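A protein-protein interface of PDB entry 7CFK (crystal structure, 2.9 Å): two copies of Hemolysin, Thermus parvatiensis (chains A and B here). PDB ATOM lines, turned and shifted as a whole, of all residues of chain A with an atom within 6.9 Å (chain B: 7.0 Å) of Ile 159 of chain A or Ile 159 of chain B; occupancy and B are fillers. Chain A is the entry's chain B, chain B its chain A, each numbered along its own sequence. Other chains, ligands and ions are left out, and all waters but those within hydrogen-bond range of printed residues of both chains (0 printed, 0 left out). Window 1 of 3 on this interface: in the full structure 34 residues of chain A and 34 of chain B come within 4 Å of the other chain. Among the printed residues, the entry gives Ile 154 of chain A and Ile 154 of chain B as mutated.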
ATOM      1  N   LEU A 129       7.593   1.863   8.989  1.00  0.00           N
ATOM      2  CA  LEU A 129       6.454   1.056   8.593  1.00  0.00           C
ATOM      3  C   LEU A 129       5.525   1.855   7.700  1.00  0.00           C
ATOM      4  O   LEU A 129       5.105   1.378   6.636  1.00  0.00           O
ATOM      5  CB  LEU A 129       5.735   0.543   9.834  1.00  0.00           C
ATOM      6  CG  LEU A 129       4.436  -0.226   9.630  1.00  0.00           C
ATOM      7  CD1 LEU A 129       4.629  -1.412   8.711  1.00  0.00           C
ATOM      8  CD2 LEU A 129       3.916  -0.686  10.998  1.00  0.00           C
ATOM      9  N   ILE A 154      14.534  -3.681   6.492  1.00  0.00           N
ATOM     10  CA  ILE A 154      13.440  -4.200   5.683  1.00  0.00           C
ATOM     11  C   ILE A 154      12.152  -4.200   6.505  1.00  0.00           C
ATOM     12  O   ILE A 154      12.158  -4.179   7.743  1.00  0.00           O
ATOM     13  CB  ILE A 154      13.722  -5.614   5.147  1.00  0.00           C
ATOM     14  CG1 ILE A 154      14.181  -6.517   6.293  1.00  0.00           C
ATOM     15  CG2 ILE A 154      14.744  -5.541   4.041  1.00  0.00           C
ATOM     16  CD1 ILE A 154      14.162  -7.968   6.006  1.00  0.00           C
ATOM     17  N   LEU A 155      11.033  -4.246   5.784  1.00  0.00           N
ATOM     18  CA  LEU A 155       9.733  -4.233   6.435  1.00  0.00           C
ATOM     19  C   LEU A 155       9.558  -5.434   7.350  1.00  0.00           C
ATOM     20  O   LEU A 155       8.950  -5.318   8.416  1.00  0.00           O
ATOM     21  CB  LEU A 155       8.652  -4.191   5.366  1.00  0.00           C
ATOM     22  CG  LEU A 155       7.201  -4.336   5.756  1.00  0.00           C
ATOM     23  CD1 LEU A 155       6.403  -3.467   4.815  1.00  0.00           C
ATOM     24  CD2 LEU A 155       6.804  -5.784   5.602  1.00  0.00           C
ATOM     25  N   GLU A 156      10.070  -6.596   6.945  1.00  0.00           N
ATOM     26  CA  GLU A 156       9.923  -7.801   7.752  1.00  0.00           C
ATOM     27  C   GLU A 156      10.565  -7.648   9.115  1.00  0.00           C
ATOM     28  O   GLU A 156      10.155  -8.327  10.057  1.00  0.00           O
ATOM     29  CB  GLU A 156      10.526  -9.008   7.034  1.00  0.00           C
ATOM     30  CG  GLU A 156       9.692  -9.513   5.886  1.00  0.00           C
ATOM     31  CD  GLU A 156       9.855  -8.668   4.625  1.00  0.00           C
ATOM     32  OE1 GLU A 156      10.775  -7.820   4.615  1.00  0.00           O
ATOM     33  OE2 GLU A 156       9.055  -8.830   3.659  1.00  0.00           O
ATOM     34  N   ASP A 157      11.541  -6.752   9.244  1.00  0.00           N
ATOM     35  CA  ASP A 157      12.142  -6.482  10.546  1.00  0.00           C
ATOM     36  C   ASP A 157      11.177  -5.731  11.465  1.00  0.00           C
ATOM     37  O   ASP A 157      10.980  -6.123  12.623  1.00  0.00           O
ATOM     38  CB  ASP A 157      13.446  -5.710  10.358  1.00  0.00           C
ATOM     39  CG  ASP A 157      14.666  -6.638  10.249  1.00  0.00           C
ATOM     40  OD1 ASP A 157      15.561  -6.356   9.413  1.00  0.00           O
ATOM     41  OD2 ASP A 157      14.728  -7.655  10.995  1.00  0.00           O
ATOM     42  N   VAL A 158      10.547  -4.664  10.954  1.00  0.00           N
ATOM     43  CA  VAL A 158       9.467  -3.991  11.680  1.00  0.00           C
ATOM     44  C   VAL A 158       8.388  -4.998  12.057  1.00  0.00           C
ATOM     45  O   VAL A 158       7.898  -5.040  13.201  1.00  0.00           O
ATOM     46  CB  VAL A 158       8.887  -2.851  10.820  1.00  0.00           C
ATOM     47  CG1 VAL A 158       7.739  -2.147  11.529  1.00  0.00           C
ATOM     48  CG2 VAL A 158       9.964  -1.863  10.438  1.00  0.00           C
ATOM     49  N   ILE A 159       8.016  -5.833  11.089  1.00  0.00           N
ATOM     50  CA  ILE A 159       7.019  -6.867  11.325  1.00  0.00           C
ATOM     51  C   ILE A 159       7.434  -7.736  12.502  1.00  0.00           C
ATOM     52  O   ILE A 159       6.655  -7.962  13.435  1.00  0.00           O
ATOM     53  CB  ILE A 159       6.827  -7.704  10.050  1.00  0.00           C
ATOM     54  CG1 ILE A 159       6.255  -6.830   8.919  1.00  0.00           C
ATOM     55  CG2 ILE A 159       6.044  -8.984  10.336  1.00  0.00           C
ATOM     56  CD1 ILE A 159       5.043  -5.967   9.291  1.00  0.00           C
ATOM     57  N   GLU A 160       8.678  -8.210  12.487  1.00  0.00           N
ATOM     58  CA  GLU A 160       9.131  -9.085  13.552  1.00  0.00           C
ATOM     59  C   GLU A 160       9.095  -8.372  14.883  1.00  0.00           C
ATOM     60  O   GLU A 160       8.830  -8.999  15.914  1.00  0.00           O
ATOM     61  CB  GLU A 160      10.541  -9.576  13.254  1.00  0.00           C
ATOM     62  CG  GLU A 160      10.614 -10.832  12.404  1.00  0.00           C
ATOM     63  CD  GLU A 160      12.018 -11.413  12.384  1.00  0.00           C
ATOM     64  OE1 GLU A 160      12.995 -10.615  12.352  1.00  0.00           O
ATOM     65  OE2 GLU A 160      12.137 -12.662  12.417  1.00  0.00           O
ATOM     66  N   GLU A 161       9.356  -7.061  14.865  1.00  0.00           N
ATOM     67  CA  GLU A 161       9.300  -6.256  16.081  1.00  0.00           C
ATOM     68  C   GLU A 161       7.924  -6.332  16.704  1.00  0.00           C
ATOM     69  O   GLU A 161       7.780  -6.495  17.922  1.00  0.00           O
ATOM     70  CB  GLU A 161       9.652  -4.806  15.762  1.00  0.00           C
ATOM     71  CG  GLU A 161      10.268  -4.082  16.926  1.00  0.00           C
ATOM     72  CD  GLU A 161      11.607  -4.693  17.329  1.00  0.00           C
ATOM     73  OE1 GLU A 161      12.177  -5.444  16.500  1.00  0.00           O
ATOM     74  OE2 GLU A 161      12.096  -4.428  18.460  1.00  0.00           O
ATOM     75  N   ILE A 162       6.901  -6.252  15.868  1.00  0.00           N
ATOM     76  CA  ILE A 162       5.537  -6.439  16.350  1.00  0.00           C
ATOM     77  C   ILE A 162       5.305  -7.877  16.827  1.00  0.00           C
ATOM     78  O   ILE A 162       4.983  -8.113  17.995  1.00  0.00           O
ATOM     79  CB  ILE A 162       4.540  -6.062  15.251  1.00  0.00           C
ATOM     80  CG1 ILE A 162       4.611  -4.570  14.995  1.00  0.00           C
ATOM     81  CG2 ILE A 162       3.176  -6.458  15.672  1.00  0.00           C
ATOM     82  CD1 ILE A 162       3.693  -4.126  13.936  1.00  0.00           C
ATOM     83  N   VAL A 163       5.445  -8.855  15.929  1.00  0.00           N
ATOM     84  CA  VAL A 163       4.928 -10.207  16.199  1.00  0.00           C
ATOM     85  C   VAL A 163       5.964 -11.091  16.876  1.00  0.00           C
ATOM     86  O   VAL A 163       5.633 -11.840  17.797  1.00  0.00           O
ATOM     87  CB  VAL A 163       4.389 -10.890  14.914  1.00  0.00           C
ATOM     88  CG1 VAL A 163       3.086 -10.285  14.490  1.00  0.00           C
ATOM     89  CG2 VAL A 163       5.361 -10.788  13.790  1.00  0.00           C
ATOM     90  N   GLY A 164       7.213 -11.039  16.438  1.00  0.00           N
ATOM     91  CA  GLY A 164       8.246 -11.930  16.908  1.00  0.00           C
ATOM     92  C   GLY A 164       9.002 -12.481  15.732  1.00  0.00           C
ATOM     93  O   GLY A 164       8.789 -12.077  14.586  1.00  0.00           O
ATOM     94  N   GLU A 165       9.907 -13.415  15.996  1.00  0.00           N
ATOM     95  CA  GLU A 165      10.715 -13.976  14.922  1.00  0.00           C
ATOM     96  C   GLU A 165       9.888 -14.975  14.120  1.00  0.00           C
ATOM     97  O   GLU A 165       9.135 -15.773  14.686  1.00  0.00           O
ATOM     98  CB  GLU A 165      11.977 -14.644  15.481  1.00  0.00           C
ATOM     99  N   ILE A 166       9.986 -14.894  12.795  1.00  0.00           N
ATOM    100  CA  ILE A 166       9.465 -15.936  11.921  1.00  0.00           C
ATOM    101  C   ILE A 166      10.501 -16.129  10.823  1.00  0.00           C
ATOM    102  O   ILE A 166      11.053 -15.146  10.318  1.00  0.00           O
ATOM    103  CB  ILE A 166       8.109 -15.590  11.265  1.00  0.00           C
ATOM    104  CG1 ILE A 166       7.070 -15.063  12.258  1.00  0.00           C
ATOM    105  CG2 ILE A 166       7.533 -16.862  10.631  1.00  0.00           C
ATOM    106  CD1 ILE A 166       7.069 -13.543  12.323  1.00  0.00           C
ATOM    107  N   LEU B  37      -8.211 -10.308  15.884  1.00  0.00           N
ATOM    108  CA  LEU B  37      -7.643 -11.534  15.313  1.00  0.00           C
ATOM    109  C   LEU B  37      -8.296 -12.786  15.894  1.00  0.00           C
ATOM    110  O   LEU B  37      -8.524 -13.760  15.171  1.00  0.00           O
ATOM    111  CB  LEU B  37      -6.133 -11.592  15.544  1.00  0.00           C
ATOM    112  CG  LEU B  37      -5.243 -10.599  14.803  1.00  0.00           C
ATOM    113  CD1 LEU B  37      -3.809 -10.641  15.349  1.00  0.00           C
ATOM    114  CD2 LEU B  37      -5.287 -10.863  13.312  1.00  0.00           C
ATOM    115  N   LEU B 129      -1.990 -17.614  13.457  1.00  0.00           N
ATOM    116  CA  LEU B 129      -0.731 -16.914  13.655  1.00  0.00           C
ATOM    117  C   LEU B 129       0.110 -17.600  14.723  1.00  0.00           C
ATOM    118  O   LEU B 129       1.338 -17.728  14.588  1.00  0.00           O
ATOM    119  CB  LEU B 129      -1.044 -15.472  14.034  1.00  0.00           C
ATOM    120  CG  LEU B 129       0.025 -14.485  14.479  1.00  0.00           C
ATOM    121  CD1 LEU B 129       0.858 -14.039  13.297  1.00  0.00           C
ATOM    122  CD2 LEU B 129      -0.610 -13.287  15.175  1.00  0.00           C
ATOM    123  N   ILE B 154      -1.648 -17.334   3.919  1.00  0.00           N
ATOM    124  CA  ILE B 154      -0.256 -17.123   4.294  1.00  0.00           C
ATOM    125  C   ILE B 154      -0.181 -16.144   5.468  1.00  0.00           C
ATOM    126  O   ILE B 154      -1.129 -15.426   5.783  1.00  0.00           O
ATOM    127  CB  ILE B 154       0.618 -16.609   3.132  1.00  0.00           C
ATOM    128  CG1 ILE B 154       0.095 -15.276   2.593  1.00  0.00           C
ATOM    129  CG2 ILE B 154       0.648 -17.623   2.036  1.00  0.00           C
ATOM    130  CD1 ILE B 154       0.914 -14.679   1.500  1.00  0.00           C
ATOM    131  N   LEU B 155       1.006 -16.104   6.081  1.00  0.00           N
ATOM    132  CA  LEU B 155       1.254 -15.255   7.240  1.00  0.00           C
ATOM    133  C   LEU B 155       1.017 -13.783   6.935  1.00  0.00           C
ATOM    134  O   LEU B 155       0.481 -13.054   7.774  1.00  0.00           O
ATOM    135  CB  LEU B 155       2.687 -15.479   7.710  1.00  0.00           C
ATOM    136  CG  LEU B 155       3.245 -14.874   8.989  1.00  0.00           C
ATOM    137  CD1 LEU B 155       2.506 -15.441  10.196  1.00  0.00           C
ATOM    138  CD2 LEU B 155       4.737 -15.204   9.046  1.00  0.00           C
ATOM    139  N   GLU B 156       1.429 -13.324   5.751  1.00  0.00           N
ATOM    140  CA  GLU B 156       1.315 -11.918   5.380  1.00  0.00           C
ATOM    141  C   GLU B 156      -0.125 -11.472   5.253  1.00  0.00           C
ATOM    142  O   GLU B 156      -0.387 -10.273   5.347  1.00  0.00           O
ATOM    143  CB  GLU B 156       2.069 -11.665   4.075  1.00  0.00           C
ATOM    144  CG  GLU B 156       3.540 -12.036   4.139  1.00  0.00           C
ATOM    145  CD  GLU B 156       3.811 -13.554   4.275  1.00  0.00           C
ATOM    146  OE1 GLU B 156       2.862 -14.349   4.419  1.00  0.00           O
ATOM    147  OE2 GLU B 156       4.989 -13.961   4.270  1.00  0.00           O
ATOM    148  N   ASP B 157      -1.048 -12.423   5.087  1.00  0.00           N
ATOM    149  CA  ASP B 157      -2.483 -12.156   5.170  1.00  0.00           C
ATOM    150  C   ASP B 157      -2.860 -11.651   6.559  1.00  0.00           C
ATOM    151  O   ASP B 157      -3.491 -10.594   6.716  1.00  0.00           O
ATOM    152  CB  ASP B 157      -3.252 -13.451   4.910  1.00  0.00           C
ATOM    153  CG  ASP B 157      -2.985 -14.028   3.538  1.00  0.00           C
ATOM    154  OD1 ASP B 157      -2.630 -13.241   2.649  1.00  0.00           O
ATOM    155  OD2 ASP B 157      -3.095 -15.269   3.351  1.00  0.00           O
ATOM    156  N   VAL B 158      -2.453 -12.407   7.574  1.00  0.00           N
ATOM    157  CA  VAL B 158      -2.677 -12.034   8.963  1.00  0.00           C
ATOM    158  C   VAL B 158      -1.959 -10.724   9.272  1.00  0.00           C
ATOM    159  O   VAL B 158      -2.495  -9.819   9.932  1.00  0.00           O
ATOM    160  CB  VAL B 158      -2.172 -13.166   9.869  1.00  0.00           C
ATOM    161  CG1 VAL B 158      -2.527 -12.920  11.313  1.00  0.00           C
ATOM    162  CG2 VAL B 158      -2.595 -14.511   9.341  1.00  0.00           C
ATOM    163  N   ILE B 159      -0.718 -10.612   8.801  1.00  0.00           N
ATOM    164  CA  ILE B 159       0.062  -9.410   9.064  1.00  0.00           C
ATOM    165  C   ILE B 159      -0.671  -8.192   8.551  1.00  0.00           C
ATOM    166  O   ILE B 159      -0.867  -7.216   9.282  1.00  0.00           O
ATOM    167  CB  ILE B 159       1.457  -9.505   8.424  1.00  0.00           C
ATOM    168  CG1 ILE B 159       2.199 -10.746   8.930  1.00  0.00           C
ATOM    169  CG2 ILE B 159       2.210  -8.225   8.668  1.00  0.00           C
ATOM    170  CD1 ILE B 159       2.178 -10.899  10.406  1.00  0.00           C
ATOM    171  N   GLU B 160      -1.104  -8.243   7.288  1.00  0.00           N
ATOM    172  CA  GLU B 160      -1.806  -7.119   6.687  1.00  0.00           C
ATOM    173  C   GLU B 160      -3.118  -6.874   7.404  1.00  0.00           C
ATOM    174  O   GLU B 160      -3.602  -5.737   7.467  1.00  0.00           O
ATOM    175  CB  GLU B 160      -2.029  -7.380   5.197  1.00  0.00           C
ATOM    176  N   GLU B 161      -3.676  -7.928   7.995  1.00  0.00           N
ATOM    177  CA  GLU B 161      -4.897  -7.807   8.774  1.00  0.00           C
ATOM    178  C   GLU B 161      -4.643  -7.068  10.077  1.00  0.00           C
ATOM    179  O   GLU B 161      -5.572  -6.491  10.655  1.00  0.00           O
ATOM    180  CB  GLU B 161      -5.424  -9.233   8.949  1.00  0.00           C
ATOM    181  CG  GLU B 161      -6.794  -9.573   9.534  1.00  0.00           C
ATOM    182  CD  GLU B 161      -7.987  -8.949   8.784  1.00  0.00           C
ATOM    183  OE1 GLU B 161      -7.820  -8.389   7.662  1.00  0.00           O
ATOM    184  OE2 GLU B 161      -9.133  -9.237   9.206  1.00  0.00           O
ATOM    185  N   ILE B 162      -3.392  -7.055  10.522  1.00  0.00           N
ATOM    186  CA  ILE B 162      -2.966  -6.204  11.632  1.00  0.00           C
ATOM    187  C   ILE B 162      -2.592  -4.797  11.175  1.00  0.00           C
ATOM    188  O   ILE B 162      -3.006  -3.812  11.792  1.00  0.00           O
ATOM    189  CB  ILE B 162      -1.806  -6.867  12.373  1.00  0.00           C
ATOM    190  CG1 ILE B 162      -2.285  -8.160  13.001  1.00  0.00           C
ATOM    191  CG2 ILE B 162      -1.288  -5.972  13.437  1.00  0.00           C
ATOM    192  CD1 ILE B 162      -1.176  -8.986  13.546  1.00  0.00           C
ATOM    193  N   VAL B 163      -1.837  -4.661  10.087  1.00  0.00           N
ATOM    194  CA  VAL B 163      -1.162  -3.406   9.763  1.00  0.00           C
ATOM    195  C   VAL B 163      -1.592  -2.776   8.445  1.00  0.00           C
ATOM    196  O   VAL B 163      -1.187  -1.638   8.172  1.00  0.00           O
ATOM    197  CB  VAL B 163       0.369  -3.581   9.763  1.00  0.00           C
ATOM    198  CG1 VAL B 163       0.822  -4.245  11.049  1.00  0.00           C
ATOM    199  CG2 VAL B 163       0.810  -4.368   8.536  1.00  0.00           C
ATOM    200  N   GLY B 164      -2.348  -3.452   7.597  1.00  0.00           N
ATOM    201  CA  GLY B 164      -2.770  -2.868   6.340  1.00  0.00           C
ATOM    202  C   GLY B 164      -2.151  -3.561   5.129  1.00  0.00           C
ATOM    203  O   GLY B 164      -1.217  -4.362   5.228  1.00  0.00           O
ATOM    204  N   GLU B 165      -2.708  -3.232   3.963  1.00  0.00           N
ATOM    205  CA  GLU B 165      -2.229  -3.823   2.722  1.00  0.00           C
ATOM    206  C   GLU B 165      -0.741  -3.534   2.554  1.00  0.00           C
ATOM    207  O   GLU B 165      -0.280  -2.416   2.794  1.00  0.00           O
ATOM    208  CB  GLU B 165      -3.024  -3.283   1.527  1.00  0.00           C
ATOM    209  N   ILE B 166       0.009  -4.558   2.168  1.00  0.00           N
ATOM    210  CA  ILE B 166       1.466  -4.476   2.047  1.00  0.00           C
ATOM    211  C   ILE B 166       1.823  -4.859   0.611  1.00  0.00           C
ATOM    212  O   ILE B 166       2.072  -6.026   0.280  1.00  0.00           O
ATOM    213  CB  ILE B 166       2.185  -5.324   3.111  1.00  0.00           C
ATOM    214  CG1 ILE B 166       1.714  -6.802   3.133  1.00  0.00           C
ATOM    215  CG2 ILE B 166       2.053  -4.672   4.493  1.00  0.00           C
ATOM    216  CD1 ILE B 166       2.530  -7.721   4.042  1.00  0.00           C
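The side-chain carboxylate of Glu 160 of chain A sits at hydrogen-bond distance from the backbone NH of Ile 166 of chain A.
Among the printed residues, pairs that only touch across the chains: Ile 166 of chain A with Leu 155 of chain B (3.6 Å) and Ile 159 of chain A with Ile 159 of chain B (3.7 Å).
Ile 159 of chain A touches just one residue of chain B: Ile 159 (3.7 Å).
Ile 159 of chain B touches just one residue of chain A: Ile 159 (3.7 Å).
Printed residues of chain B within 4 Å of Ile 166 of chain A: Leu 155 (3.6 Å).
Of the printed residues of chain A, Leu 155 of chain B touches Ile 166.
Leu 129 of chain B touches none of the printed residues of chain A.
The nearest residue of chain A that does not touch Ile 159 of chain B is Val 163 of chain A (4.2 Å).
Printed residues of chain A that touch a printed residue of chain B: Ile 159 and Ile 166.
Hydrophobic or aromatic side chains of chain A that line the printed part of chain B: Ile 159 and Ile 166.
Of the 15 printed residues of chain B, 2 touch a printed residue of chain A.
Printed residues of chain B that touch a printed residue of chain A: Leu 155 and Ile 159.
Hydrophobic or aromatic side chains of chain B that line the printed part of chain A: Leu 155 and Ile 159.
Among the printed residues, 2 pairs touch across the chains.
Among the printed residues, no Asp or Glu carboxylate lies within 4 Å of a Lys or Arg side-chain nitrogen of the other chain.
Ile 159 of chain A touches its own counterpart, Ile 159 of chain B.
Ile 166 of chain A touches Leu 155 of chain B, but with the chains exchanged Leu 155 of chain A does not touch Ile 166 of chain B (4.5 Å).
Positions printed for both chains: 129, 154, 155, 156, 157, 158, 159, 160, 161, 162, 163, 164, 165 and 166.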
